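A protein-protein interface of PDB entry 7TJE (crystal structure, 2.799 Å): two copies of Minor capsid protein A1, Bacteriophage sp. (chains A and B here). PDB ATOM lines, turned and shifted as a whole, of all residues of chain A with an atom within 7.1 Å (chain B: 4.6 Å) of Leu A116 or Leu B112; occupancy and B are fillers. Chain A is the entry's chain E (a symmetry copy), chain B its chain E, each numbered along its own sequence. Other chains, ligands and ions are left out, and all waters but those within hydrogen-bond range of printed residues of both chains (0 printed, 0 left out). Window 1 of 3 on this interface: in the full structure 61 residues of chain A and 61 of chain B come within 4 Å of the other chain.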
ATOM      1  N   LEU A   8       8.292 -36.511 -13.467  1.00  0.00           N
ATOM      2  CA  LEU A   8       7.795 -36.192 -12.142  1.00  0.00           C
ATOM      3  C   LEU A   8       6.361 -36.669 -12.014  1.00  0.00           C
ATOM      4  O   LEU A   8       5.563 -36.497 -12.934  1.00  0.00           O
ATOM      5  CB  LEU A   8       7.881 -34.690 -11.888  1.00  0.00           C
ATOM      6  CG  LEU A   8       9.249 -34.113 -12.221  1.00  0.00           C
ATOM      7  CD1 LEU A   8       9.247 -32.623 -12.004  1.00  0.00           C
ATOM      8  CD2 LEU A   8      10.332 -34.765 -11.394  1.00  0.00           C
ATOM      9  N   ILE A  11       1.908 -34.552  -9.147  1.00  0.00           N
ATOM     10  CA  ILE A  11       2.041 -33.137  -8.841  1.00  0.00           C
ATOM     11  C   ILE A  11       0.738 -32.437  -9.205  1.00  0.00           C
ATOM     12  O   ILE A  11      -0.228 -33.086  -9.625  1.00  0.00           O
ATOM     13  CB  ILE A  11       3.248 -32.539  -9.576  1.00  0.00           C
ATOM     14  CG1 ILE A  11       2.960 -32.394 -11.061  1.00  0.00           C
ATOM     15  CG2 ILE A  11       4.445 -33.430  -9.388  1.00  0.00           C
ATOM     16  CD1 ILE A  11       4.201 -32.106 -11.862  1.00  0.00           C
ATOM     17  N   VAL A  66      18.562 -24.287  -8.779  1.00  0.00           N
ATOM     18  CA  VAL A  66      17.475 -24.857  -9.568  1.00  0.00           C
ATOM     19  C   VAL A  66      16.488 -23.754  -9.912  1.00  0.00           C
ATOM     20  O   VAL A  66      16.182 -22.904  -9.071  1.00  0.00           O
ATOM     21  CB  VAL A  66      16.759 -25.990  -8.818  1.00  0.00           C
ATOM     22  CG1 VAL A  66      15.717 -26.612  -9.708  1.00  0.00           C
ATOM     23  CG2 VAL A  66      17.751 -27.014  -8.366  1.00  0.00           C
ATOM     24  N   LYS A  67      15.989 -23.771 -11.145  1.00  0.00           N
ATOM     25  CA  LYS A  67      15.082 -22.752 -11.655  1.00  0.00           C
ATOM     26  C   LYS A  67      13.940 -23.413 -12.409  1.00  0.00           C
ATOM     27  O   LYS A  67      14.180 -24.203 -13.324  1.00  0.00           O
ATOM     28  CB  LYS A  67      15.806 -21.796 -12.594  1.00  0.00           C
ATOM     29  CG  LYS A  67      16.520 -20.653 -11.948  1.00  0.00           C
ATOM     30  CD  LYS A  67      17.519 -20.044 -12.932  1.00  0.00           C
ATOM     31  CE  LYS A  67      17.758 -18.557 -12.661  1.00  0.00           C
ATOM     32  NZ  LYS A  67      18.933 -18.365 -11.750  1.00  0.00           N
ATOM     33  N   ILE A  68      12.704 -23.079 -12.045  1.00  0.00           N
ATOM     34  CA  ILE A  68      11.502 -23.510 -12.762  1.00  0.00           C
ATOM     35  C   ILE A  68      10.903 -22.285 -13.427  1.00  0.00           C
ATOM     36  O   ILE A  68      10.776 -21.236 -12.791  1.00  0.00           O
ATOM     37  CB  ILE A  68      10.477 -24.154 -11.813  1.00  0.00           C
ATOM     38  CG1 ILE A  68      11.064 -25.413 -11.169  1.00  0.00           C
ATOM     39  CG2 ILE A  68       9.163 -24.440 -12.540  1.00  0.00           C
ATOM     40  CD1 ILE A  68      10.162 -26.053 -10.176  1.00  0.00           C
ATOM     41  N   ALA A  90      10.068 -20.440  -9.943  1.00  0.00           N
ATOM     42  CA  ALA A  90      10.729 -20.832  -8.713  1.00  0.00           C
ATOM     43  C   ALA A  90      12.235 -20.700  -8.911  1.00  0.00           C
ATOM     44  O   ALA A  90      12.757 -20.827 -10.028  1.00  0.00           O
ATOM     45  CB  ALA A  90      10.360 -22.265  -8.299  1.00  0.00           C
ATOM     46  N   ASP A  91      12.932 -20.426  -7.818  1.00  0.00           N
ATOM     47  CA  ASP A  91      14.374 -20.262  -7.884  1.00  0.00           C
ATOM     48  C   ASP A  91      14.893 -20.684  -6.524  1.00  0.00           C
ATOM     49  O   ASP A  91      14.630 -19.998  -5.541  1.00  0.00           O
ATOM     50  CB  ASP A  91      14.736 -18.817  -8.221  1.00  0.00           C
ATOM     51  CG  ASP A  91      16.231 -18.594  -8.371  1.00  0.00           C
ATOM     52  OD1 ASP A  91      17.044 -19.180  -7.599  1.00  0.00           O
ATOM     53  OD2 ASP A  91      16.583 -17.837  -9.308  1.00  0.00           O
ATOM     54  N   VAL A  92      15.589 -21.813  -6.453  1.00  0.00           N
ATOM     55  CA  VAL A  92      16.222 -22.238  -5.211  1.00  0.00           C
ATOM     56  C   VAL A  92      17.734 -22.315  -5.408  1.00  0.00           C
ATOM     57  O   VAL A  92      18.218 -22.874  -6.397  1.00  0.00           O
ATOM     58  CB  VAL A  92      15.657 -23.571  -4.694  1.00  0.00           C
ATOM     59  CG1 VAL A  92      15.858 -24.653  -5.686  1.00  0.00           C
ATOM     60  CG2 VAL A  92      16.346 -23.943  -3.429  1.00  0.00           C
ATOM     61  N   PHE A  94      20.995 -23.643  -3.105  1.00  0.00           N
ATOM     62  CA  PHE A  94      21.574 -24.268  -1.927  1.00  0.00           C
ATOM     63  C   PHE A  94      23.006 -23.784  -1.747  1.00  0.00           C
ATOM     64  O   PHE A  94      23.743 -23.634  -2.724  1.00  0.00           O
ATOM     65  CB  PHE A  94      21.554 -25.786  -2.078  1.00  0.00           C
ATOM     66  CG  PHE A  94      20.189 -26.352  -2.310  1.00  0.00           C
ATOM     67  CD1 PHE A  94      19.662 -26.418  -3.581  1.00  0.00           C
ATOM     68  CD2 PHE A  94      19.426 -26.813  -1.251  1.00  0.00           C
ATOM     69  CE1 PHE A  94      18.402 -26.943  -3.803  1.00  0.00           C
ATOM     70  CE2 PHE A  94      18.165 -27.333  -1.464  1.00  0.00           C
ATOM     71  CZ  PHE A  94      17.654 -27.393  -2.743  1.00  0.00           C
ATOM     72  N   THR A 110      15.857 -33.078   1.301  1.00  0.00           N
ATOM     73  CA  THR A 110      14.617 -33.744   1.677  1.00  0.00           C
ATOM     74  C   THR A 110      13.776 -32.866   2.599  1.00  0.00           C
ATOM     75  O   THR A 110      12.544 -32.963   2.578  1.00  0.00           O
ATOM     76  CB  THR A 110      14.927 -35.099   2.316  1.00  0.00           C
ATOM     77  OG1 THR A 110      15.753 -34.914   3.473  1.00  0.00           O
ATOM     78  CG2 THR A 110      15.679 -35.994   1.315  1.00  0.00           C
ATOM     79  N   GLU A 111      14.408 -31.973   3.376  1.00  0.00           N
ATOM     80  CA  GLU A 111      13.639 -31.100   4.262  1.00  0.00           C
ATOM     81  C   GLU A 111      12.839 -30.082   3.470  1.00  0.00           C
ATOM     82  O   GLU A 111      11.637 -29.930   3.684  1.00  0.00           O
ATOM     83  CB  GLU A 111      14.552 -30.381   5.256  1.00  0.00           C
ATOM     84  CG  GLU A 111      13.838 -29.286   6.040  1.00  0.00           C
ATOM     85  CD  GLU A 111      14.783 -28.387   6.817  1.00  0.00           C
ATOM     86  OE1 GLU A 111      14.299 -27.414   7.455  1.00  0.00           O
ATOM     87  OE2 GLU A 111      16.008 -28.647   6.790  1.00  0.00           O
ATOM     88  N   LEU A 112      13.496 -29.362   2.561  1.00  0.00           N
ATOM     89  CA  LEU A 112      12.782 -28.467   1.657  1.00  0.00           C
ATOM     90  C   LEU A 112      11.623 -29.184   0.956  1.00  0.00           C
ATOM     91  O   LEU A 112      10.497 -28.659   0.901  1.00  0.00           O
ATOM     92  CB  LEU A 112      13.760 -27.872   0.634  1.00  0.00           C
ATOM     93  CG  LEU A 112      13.205 -26.919  -0.419  1.00  0.00           C
ATOM     94  CD1 LEU A 112      12.366 -25.856   0.253  1.00  0.00           C
ATOM     95  CD2 LEU A 112      14.335 -26.279  -1.187  1.00  0.00           C
ATOM     96  N   ALA A 113      11.872 -30.393   0.431  1.00  0.00           N
ATOM     97  CA  ALA A 113      10.816 -31.143  -0.247  1.00  0.00           C
ATOM     98  C   ALA A 113       9.631 -31.400   0.680  1.00  0.00           C
ATOM     99  O   ALA A 113       8.485 -31.099   0.333  1.00  0.00           O
ATOM    100  CB  ALA A 113      11.366 -32.458  -0.787  1.00  0.00           C
ATOM    101  N   ALA A 114       9.883 -31.966   1.865  1.00  0.00           N
ATOM    102  CA  ALA A 114       8.786 -32.241   2.786  1.00  0.00           C
ATOM    103  C   ALA A 114       8.105 -30.962   3.213  1.00  0.00           C
ATOM    104  O   ALA A 114       6.881 -30.930   3.389  1.00  0.00           O
ATOM    105  CB  ALA A 114       9.294 -32.993   4.010  1.00  0.00           C
ATOM    106  N   LEU A 115       8.883 -29.898   3.359  1.00  0.00           N
ATOM    107  CA  LEU A 115       8.336 -28.590   3.698  1.00  0.00           C
ATOM    108  C   LEU A 115       7.335 -28.125   2.651  1.00  0.00           C
ATOM    109  O   LEU A 115       6.245 -27.648   2.987  1.00  0.00           O
ATOM    110  CB  LEU A 115       9.486 -27.589   3.831  1.00  0.00           C
ATOM    111  CG  LEU A 115       9.343 -26.292   4.609  1.00  0.00           C
ATOM    112  CD1 LEU A 115       8.865 -26.576   6.013  1.00  0.00           C
ATOM    113  CD2 LEU A 115      10.690 -25.598   4.638  1.00  0.00           C
ATOM    114  N   LEU A 116       7.679 -28.274   1.372  1.00  0.00           N
ATOM    115  CA  LEU A 116       6.797 -27.813   0.311  1.00  0.00           C
ATOM    116  C   LEU A 116       5.437 -28.515   0.325  1.00  0.00           C
ATOM    117  O   LEU A 116       4.500 -28.015  -0.305  1.00  0.00           O
ATOM    118  CB  LEU A 116       7.488 -27.987  -1.042  1.00  0.00           C
ATOM    119  CG  LEU A 116       8.678 -27.048  -1.317  1.00  0.00           C
ATOM    120  CD1 LEU A 116       9.478 -27.475  -2.554  1.00  0.00           C
ATOM    121  CD2 LEU A 116       8.250 -25.592  -1.442  1.00  0.00           C
ATOM    122  N   ALA A 117       5.279 -29.623   1.052  1.00  0.00           N
ATOM    123  CA  ALA A 117       4.005 -30.322   1.083  1.00  0.00           C
ATOM    124  C   ALA A 117       3.214 -30.057   2.359  1.00  0.00           C
ATOM    125  O   ALA A 117       2.273 -30.799   2.658  1.00  0.00           O
ATOM    126  CB  ALA A 117       4.222 -31.819   0.907  1.00  0.00           C
ATOM    127  N   SER A 118       3.566 -29.002   3.113  1.00  0.00           N
ATOM    128  CA  SER A 118       3.044 -28.746   4.448  1.00  0.00           C
ATOM    129  C   SER A 118       1.991 -27.649   4.418  1.00  0.00           C
ATOM    130  O   SER A 118       2.061 -26.752   3.574  1.00  0.00           O
ATOM    131  CB  SER A 118       4.175 -28.323   5.397  1.00  0.00           C
ATOM    132  OG  SER A 118       4.503 -26.947   5.210  1.00  0.00           O
ATOM    133  N   PRO A 119       1.033 -27.678   5.356  1.00  0.00           N
ATOM    134  CA  PRO A 119      -0.048 -26.677   5.326  1.00  0.00           C
ATOM    135  C   PRO A 119       0.458 -25.241   5.304  1.00  0.00           C
ATOM    136  O   PRO A 119      -0.062 -24.415   4.538  1.00  0.00           O
ATOM    137  CB  PRO A 119      -0.846 -26.990   6.602  1.00  0.00           C
ATOM    138  CG  PRO A 119      -0.547 -28.406   6.894  1.00  0.00           C
ATOM    139  CD  PRO A 119       0.864 -28.645   6.454  1.00  0.00           C
ATOM    140  N   LEU A 121       3.153 -24.061   3.961  1.00  0.00           N
ATOM    141  CA  LEU A 121       3.630 -23.679   2.633  1.00  0.00           C
ATOM    142  C   LEU A 121       2.542 -23.779   1.574  1.00  0.00           C
ATOM    143  O   LEU A 121       2.524 -22.966   0.640  1.00  0.00           O
ATOM    144  CB  LEU A 121       4.831 -24.524   2.208  1.00  0.00           C
ATOM    145  CG  LEU A 121       6.230 -24.111   2.674  1.00  0.00           C
ATOM    146  CD1 LEU A 121       6.482 -22.681   2.239  1.00  0.00           C
ATOM    147  CD2 LEU A 121       6.437 -24.283   4.184  1.00  0.00           C
ATOM    148  N   ILE A 122       1.646 -24.762   1.681  1.00  0.00           N
ATOM    149  CA  ILE A 122       0.491 -24.800   0.796  1.00  0.00           C
ATOM    150  C   ILE A 122      -0.281 -23.484   0.865  1.00  0.00           C
ATOM    151  O   ILE A 122      -0.640 -22.905  -0.161  1.00  0.00           O
ATOM    152  CB  ILE A 122      -0.392 -26.006   1.143  1.00  0.00           C
ATOM    153  CG1 ILE A 122       0.261 -27.291   0.633  1.00  0.00           C
ATOM    154  CG2 ILE A 122      -1.781 -25.829   0.556  1.00  0.00           C
ATOM    155  CD1 ILE A 122      -0.187 -28.533   1.346  1.00  0.00           C
ATOM    156  N   ILE A 125       2.048 -20.476  -0.694  1.00  0.00           N
ATOM    157  CA  ILE A 125       2.306 -20.512  -2.123  1.00  0.00           C
ATOM    158  C   ILE A 125       1.011 -20.595  -2.916  1.00  0.00           C
ATOM    159  O   ILE A 125       0.779 -19.780  -3.811  1.00  0.00           O
ATOM    160  CB  ILE A 125       3.264 -21.673  -2.466  1.00  0.00           C
ATOM    161  CG1 ILE A 125       4.658 -21.373  -1.928  1.00  0.00           C
ATOM    162  CG2 ILE A 125       3.367 -21.857  -3.976  1.00  0.00           C
ATOM    163  CD1 ILE A 125       5.522 -22.609  -1.704  1.00  0.00           C
ATOM    164  N   ASP A 126       0.136 -21.553  -2.587  1.00  0.00           N
ATOM    165  CA  ASP A 126      -1.068 -21.768  -3.394  1.00  0.00           C
ATOM    166  C   ASP A 126      -2.098 -20.659  -3.182  1.00  0.00           C
ATOM    167  O   ASP A 126      -2.735 -20.212  -4.141  1.00  0.00           O
ATOM    168  CB  ASP A 126      -1.683 -23.136  -3.097  1.00  0.00           C
ATOM    169  CG  ASP A 126      -0.729 -24.287  -3.392  1.00  0.00           C
ATOM    170  OD1 ASP A 126       0.434 -24.026  -3.771  1.00  0.00           O
ATOM    171  OD2 ASP A 126      -1.135 -25.460  -3.245  1.00  0.00           O
ATOM    172  N   VAL B  92      14.662 -20.528  -1.454  1.00  0.00           N
ATOM    173  CA  VAL B  92      13.796 -20.544  -2.626  1.00  0.00           C
ATOM    174  C   VAL B  92      12.895 -19.311  -2.612  1.00  0.00           C
ATOM    175  O   VAL B  92      12.293 -18.976  -1.588  1.00  0.00           O
ATOM    176  CB  VAL B  92      12.971 -21.838  -2.725  1.00  0.00           C
ATOM    177  CG1 VAL B  92      12.107 -22.010  -1.533  1.00  0.00           C
ATOM    178  CG2 VAL B  92      12.113 -21.787  -3.939  1.00  0.00           C
ATOM    179  N   PHE B  94       9.658 -17.937  -4.923  1.00  0.00           N
ATOM    180  CA  PHE B  94       8.669 -18.088  -5.977  1.00  0.00           C
ATOM    181  C   PHE B  94       8.220 -16.713  -6.454  1.00  0.00           C
ATOM    182  O   PHE B  94       8.046 -15.798  -5.645  1.00  0.00           O
ATOM    183  CB  PHE B  94       7.469 -18.876  -5.460  1.00  0.00           C
ATOM    184  CG  PHE B  94       7.820 -20.227  -4.923  1.00  0.00           C
ATOM    185  CD1 PHE B  94       8.232 -20.380  -3.617  1.00  0.00           C
ATOM    186  CD2 PHE B  94       7.747 -21.349  -5.730  1.00  0.00           C
ATOM    187  CE1 PHE B  94       8.555 -21.627  -3.114  1.00  0.00           C
ATOM    188  CE2 PHE B  94       8.073 -22.596  -5.237  1.00  0.00           C
ATOM    189  CZ  PHE B  94       8.481 -22.731  -3.927  1.00  0.00           C
ATOM    190  N   VAL B 108       3.851 -25.259  -9.620  1.00  0.00           N
ATOM    191  CA  VAL B 108       5.250 -24.922  -9.375  1.00  0.00           C
ATOM    192  C   VAL B 108       5.705 -25.470  -8.026  1.00  0.00           C
ATOM    193  O   VAL B 108       6.851 -25.904  -7.876  1.00  0.00           O
ATOM    194  CB  VAL B 108       5.461 -23.398  -9.475  1.00  0.00           C
ATOM    195  CG1 VAL B 108       6.792 -23.013  -8.937  1.00  0.00           C
ATOM    196  CG2 VAL B 108       5.386 -22.949 -10.898  1.00  0.00           C
ATOM    197  N   ARG B 109       4.823 -25.469  -7.025  1.00  0.00           N
ATOM    198  CA  ARG B 109       5.218 -25.972  -5.711  1.00  0.00           C
ATOM    199  C   ARG B 109       5.400 -27.479  -5.745  1.00  0.00           C
ATOM    200  O   ARG B 109       6.456 -28.001  -5.360  1.00  0.00           O
ATOM    201  CB  ARG B 109       4.179 -25.581  -4.653  1.00  0.00           C
ATOM    202  CG  ARG B 109       4.374 -26.203  -3.249  1.00  0.00           C
ATOM    203  CD  ARG B 109       3.193 -25.905  -2.334  1.00  0.00           C
ATOM    204  NE  ARG B 109       1.914 -26.388  -2.865  1.00  0.00           N
ATOM    205  CZ  ARG B 109       1.422 -27.615  -2.677  1.00  0.00           C
ATOM    206  NH1 ARG B 109       2.101 -28.519  -1.982  1.00  0.00           N
ATOM    207  NH2 ARG B 109       0.247 -27.946  -3.199  1.00  0.00           N
ATOM    208  N   THR B 110       4.380 -28.201  -6.197  1.00  0.00           N
ATOM    209  CA  THR B 110       4.500 -29.652  -6.236  1.00  0.00           C
ATOM    210  C   THR B 110       5.574 -30.091  -7.228  1.00  0.00           C
ATOM    211  O   THR B 110       6.201 -31.136  -7.026  1.00  0.00           O
ATOM    212  CB  THR B 110       3.142 -30.278  -6.560  1.00  0.00           C
ATOM    213  OG1 THR B 110       2.671 -29.793  -7.824  1.00  0.00           O
ATOM    214  CG2 THR B 110       2.116 -29.902  -5.477  1.00  0.00           C
ATOM    215  N   GLU B 111       5.836 -29.292  -8.274  1.00  0.00           N
ATOM    216  CA  GLU B 111       6.869 -29.666  -9.240  1.00  0.00           C
ATOM    217  C   GLU B 111       8.253 -29.580  -8.623  1.00  0.00           C
ATOM    218  O   GLU B 111       9.036 -30.525  -8.711  1.00  0.00           O
ATOM    219  CB  GLU B 111       6.801 -28.786 -10.488  1.00  0.00           C
ATOM    220  CG  GLU B 111       7.996 -28.973 -11.417  1.00  0.00           C
ATOM    221  CD  GLU B 111       8.085 -27.917 -12.505  1.00  0.00           C
ATOM    222  OE1 GLU B 111       9.068 -27.946 -13.292  1.00  0.00           O
ATOM    223  OE2 GLU B 111       7.177 -27.056 -12.572  1.00  0.00           O
ATOM    224  N   LEU B 112       8.578 -28.442  -8.010  1.00  0.00           N
ATOM    225  CA  LEU B 112       9.828 -28.323  -7.267  1.00  0.00           C
ATOM    226  C   LEU B 112      10.000 -29.474  -6.268  1.00  0.00           C
ATOM    227  O   LEU B 112      11.075 -30.094  -6.199  1.00  0.00           O
ATOM    228  CB  LEU B 112       9.883 -26.964  -6.554  1.00  0.00           C
ATOM    229  CG  LEU B 112      11.108 -26.650  -5.703  1.00  0.00           C
ATOM    230  CD1 LEU B 112      12.362 -26.928  -6.500  1.00  0.00           C
ATOM    231  CD2 LEU B 112      11.081 -25.206  -5.266  1.00  0.00           C
ATOM    232  N   ALA B 113       8.945 -29.788  -5.501  1.00  0.00           N
ATOM    233  CA  ALA B 113       9.028 -30.879  -4.531  1.00  0.00           C
ATOM    234  C   ALA B 113       9.377 -32.201  -5.207  1.00  0.00           C
ATOM    235  O   ALA B 113      10.321 -32.885  -4.799  1.00  0.00           O
ATOM    236  CB  ALA B 113       7.717 -31.001  -3.762  1.00  0.00           C
ATOM    237  N   ALA B 114       8.622 -32.587  -6.241  1.00  0.00           N
ATOM    238  CA  ALA B 114       8.907 -33.848  -6.918  1.00  0.00           C
ATOM    239  C   ALA B 114      10.278 -33.822  -7.552  1.00  0.00           C
ATOM    240  O   ALA B 114      10.981 -34.840  -7.571  1.00  0.00           O
ATOM    241  CB  ALA B 114       7.849 -34.135  -7.976  1.00  0.00           C
ATOM    242  N   LEU B 115      10.677 -32.661  -8.051  1.00  0.00           N
ATOM    243  CA  LEU B 115      12.006 -32.489  -8.626  1.00  0.00           C
ATOM    244  C   LEU B 115      13.090 -32.799  -7.603  1.00  0.00           C
ATOM    245  O   LEU B 115      14.056 -33.509  -7.903  1.00  0.00           O
ATOM    246  CB  LEU B 115      12.143 -31.057  -9.146  1.00  0.00           C
ATOM    247  CG  LEU B 115      13.176 -30.672 -10.191  1.00  0.00           C
ATOM    248  CD1 LEU B 115      13.037 -31.552 -11.410  1.00  0.00           C
ATOM    249  CD2 LEU B 115      12.965 -29.217 -10.562  1.00  0.00           C
ATOM    250  N   LEU B 116      12.937 -32.287  -6.382  1.00  0.00           N
ATOM    251  CA  LEU B 116      13.952 -32.498  -5.361  1.00  0.00           C
ATOM    252  C   LEU B 116      14.158 -33.978  -5.029  1.00  0.00           C
ATOM    253  O   LEU B 116      15.180 -34.317  -4.424  1.00  0.00           O
ATOM    254  CB  LEU B 116      13.590 -31.701  -4.107  1.00  0.00           C
ATOM    255  CG  LEU B 116      13.706 -30.169  -4.225  1.00  0.00           C
ATOM    256  CD1 LEU B 116      13.062 -29.446  -3.035  1.00  0.00           C
ATOM    257  CD2 LEU B 116      15.147 -29.710  -4.404  1.00  0.00           C
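O of Leu A116 is in hydrogen-bond range of NH1 of Arg B109 (3.0 Å).
The guanidinium group (NH2) of Arg B109 lies within salt-bridge range of the side-chain carboxylate (OD2) of Asp A126, 2.8 Å away.
Of the 11 printed residues of chain B, 11 touch a printed residue of chain A.
Printed residues of chain B that touch a printed residue of chain A: Val B92, Phe B94, Val B108, Arg B109, Thr B110, Glu B111, Leu B112, Ala B113, Ala B114, Leu B115 and Leu B116.
Hydrophobic or aromatic side chains of chain B that line the printed part of chain A: Val B92, Phe B94, Val B108, Leu B112, Ala B114, Leu B115 and Leu B116.
Along chain B the printed residues that touch a printed residue of chain A span positions 92 to 116.
Among the printed residues, 23 pairs touch across the chains.
Val B92 touches its own counterpart, Val A92.
Phe A94 touches Leu B116, and with the chains exchanged Leu A116 touches Phe B94.
Leu A112 touches Leu B116, and with the chains exchanged Leu A116 touches Leu B112.
Ala A113 touches Leu B116, and with the chains exchanged Leu A116 touches Ala B113.
Positions printed for both chains: 92, 94, 110, 111, 112, 113, 114, 115 and 116.
The backbone NH of Val A66 lies within hydrogen-bond range of the backbone carbonyl oxygen of Val A92, at 2.8 Å.
The side-chain carboxylate (OD2) of Asp A91 lies within salt-bridge range of the side-chain amino group (NZ) of Lys A67.
The backbone carbonyl oxygen of Ala A90 sits at hydrogen-bond distance from the backbone NH of Ile A68, 3.0 Å away.
Of chain B, only Phe B94, Arg B109, Leu B112 and Ala B113 come within 4 Å of Leu A116.
Leu B112 touches two residues of chain A.
Printed residues of chain B within 4 Å of Asp A91: Val B92 (3.1 Å).
Printed residues of chain A within 4 Å of Glu B111: Leu A8 and Ile A68.
Of the printed residues of chain A, Leu B116 touches Phe A94 (3.8 Å), Leu A112 (3.6 Å) and Ala A113 (3.8 Å).
Thr A110 touches none of the printed residues of chain B.
The nearest residue of chain B that does not touch Leu A116 is Leu B116 (4.1 Å).
Among the printed residues, merely in contact across the chains: Leu A8 with Glu B111, Leu A8 with Ala B114, Leu A8 with Leu B115, Ile A11 with Thr B110, Ile A11 with Ala B114, Val A66 with Leu B115, Ile A68 with Glu B111, Ile A68 with Leu B112, Ala A90 with Phe B94, Ala A90 with Val B108, Asp A91 with Val B92, Val A92 with Val B92, Phe A94 with Leu B116, Leu A112 with Leu B116, Ala A113 with Leu B116, Leu A116 with Phe B94, Leu A116 with Leu B112, Leu A116 with Ala B113, Ile A122 with Arg B109, Ile A125 with Phe B94 and Ile A125 with Arg B109.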
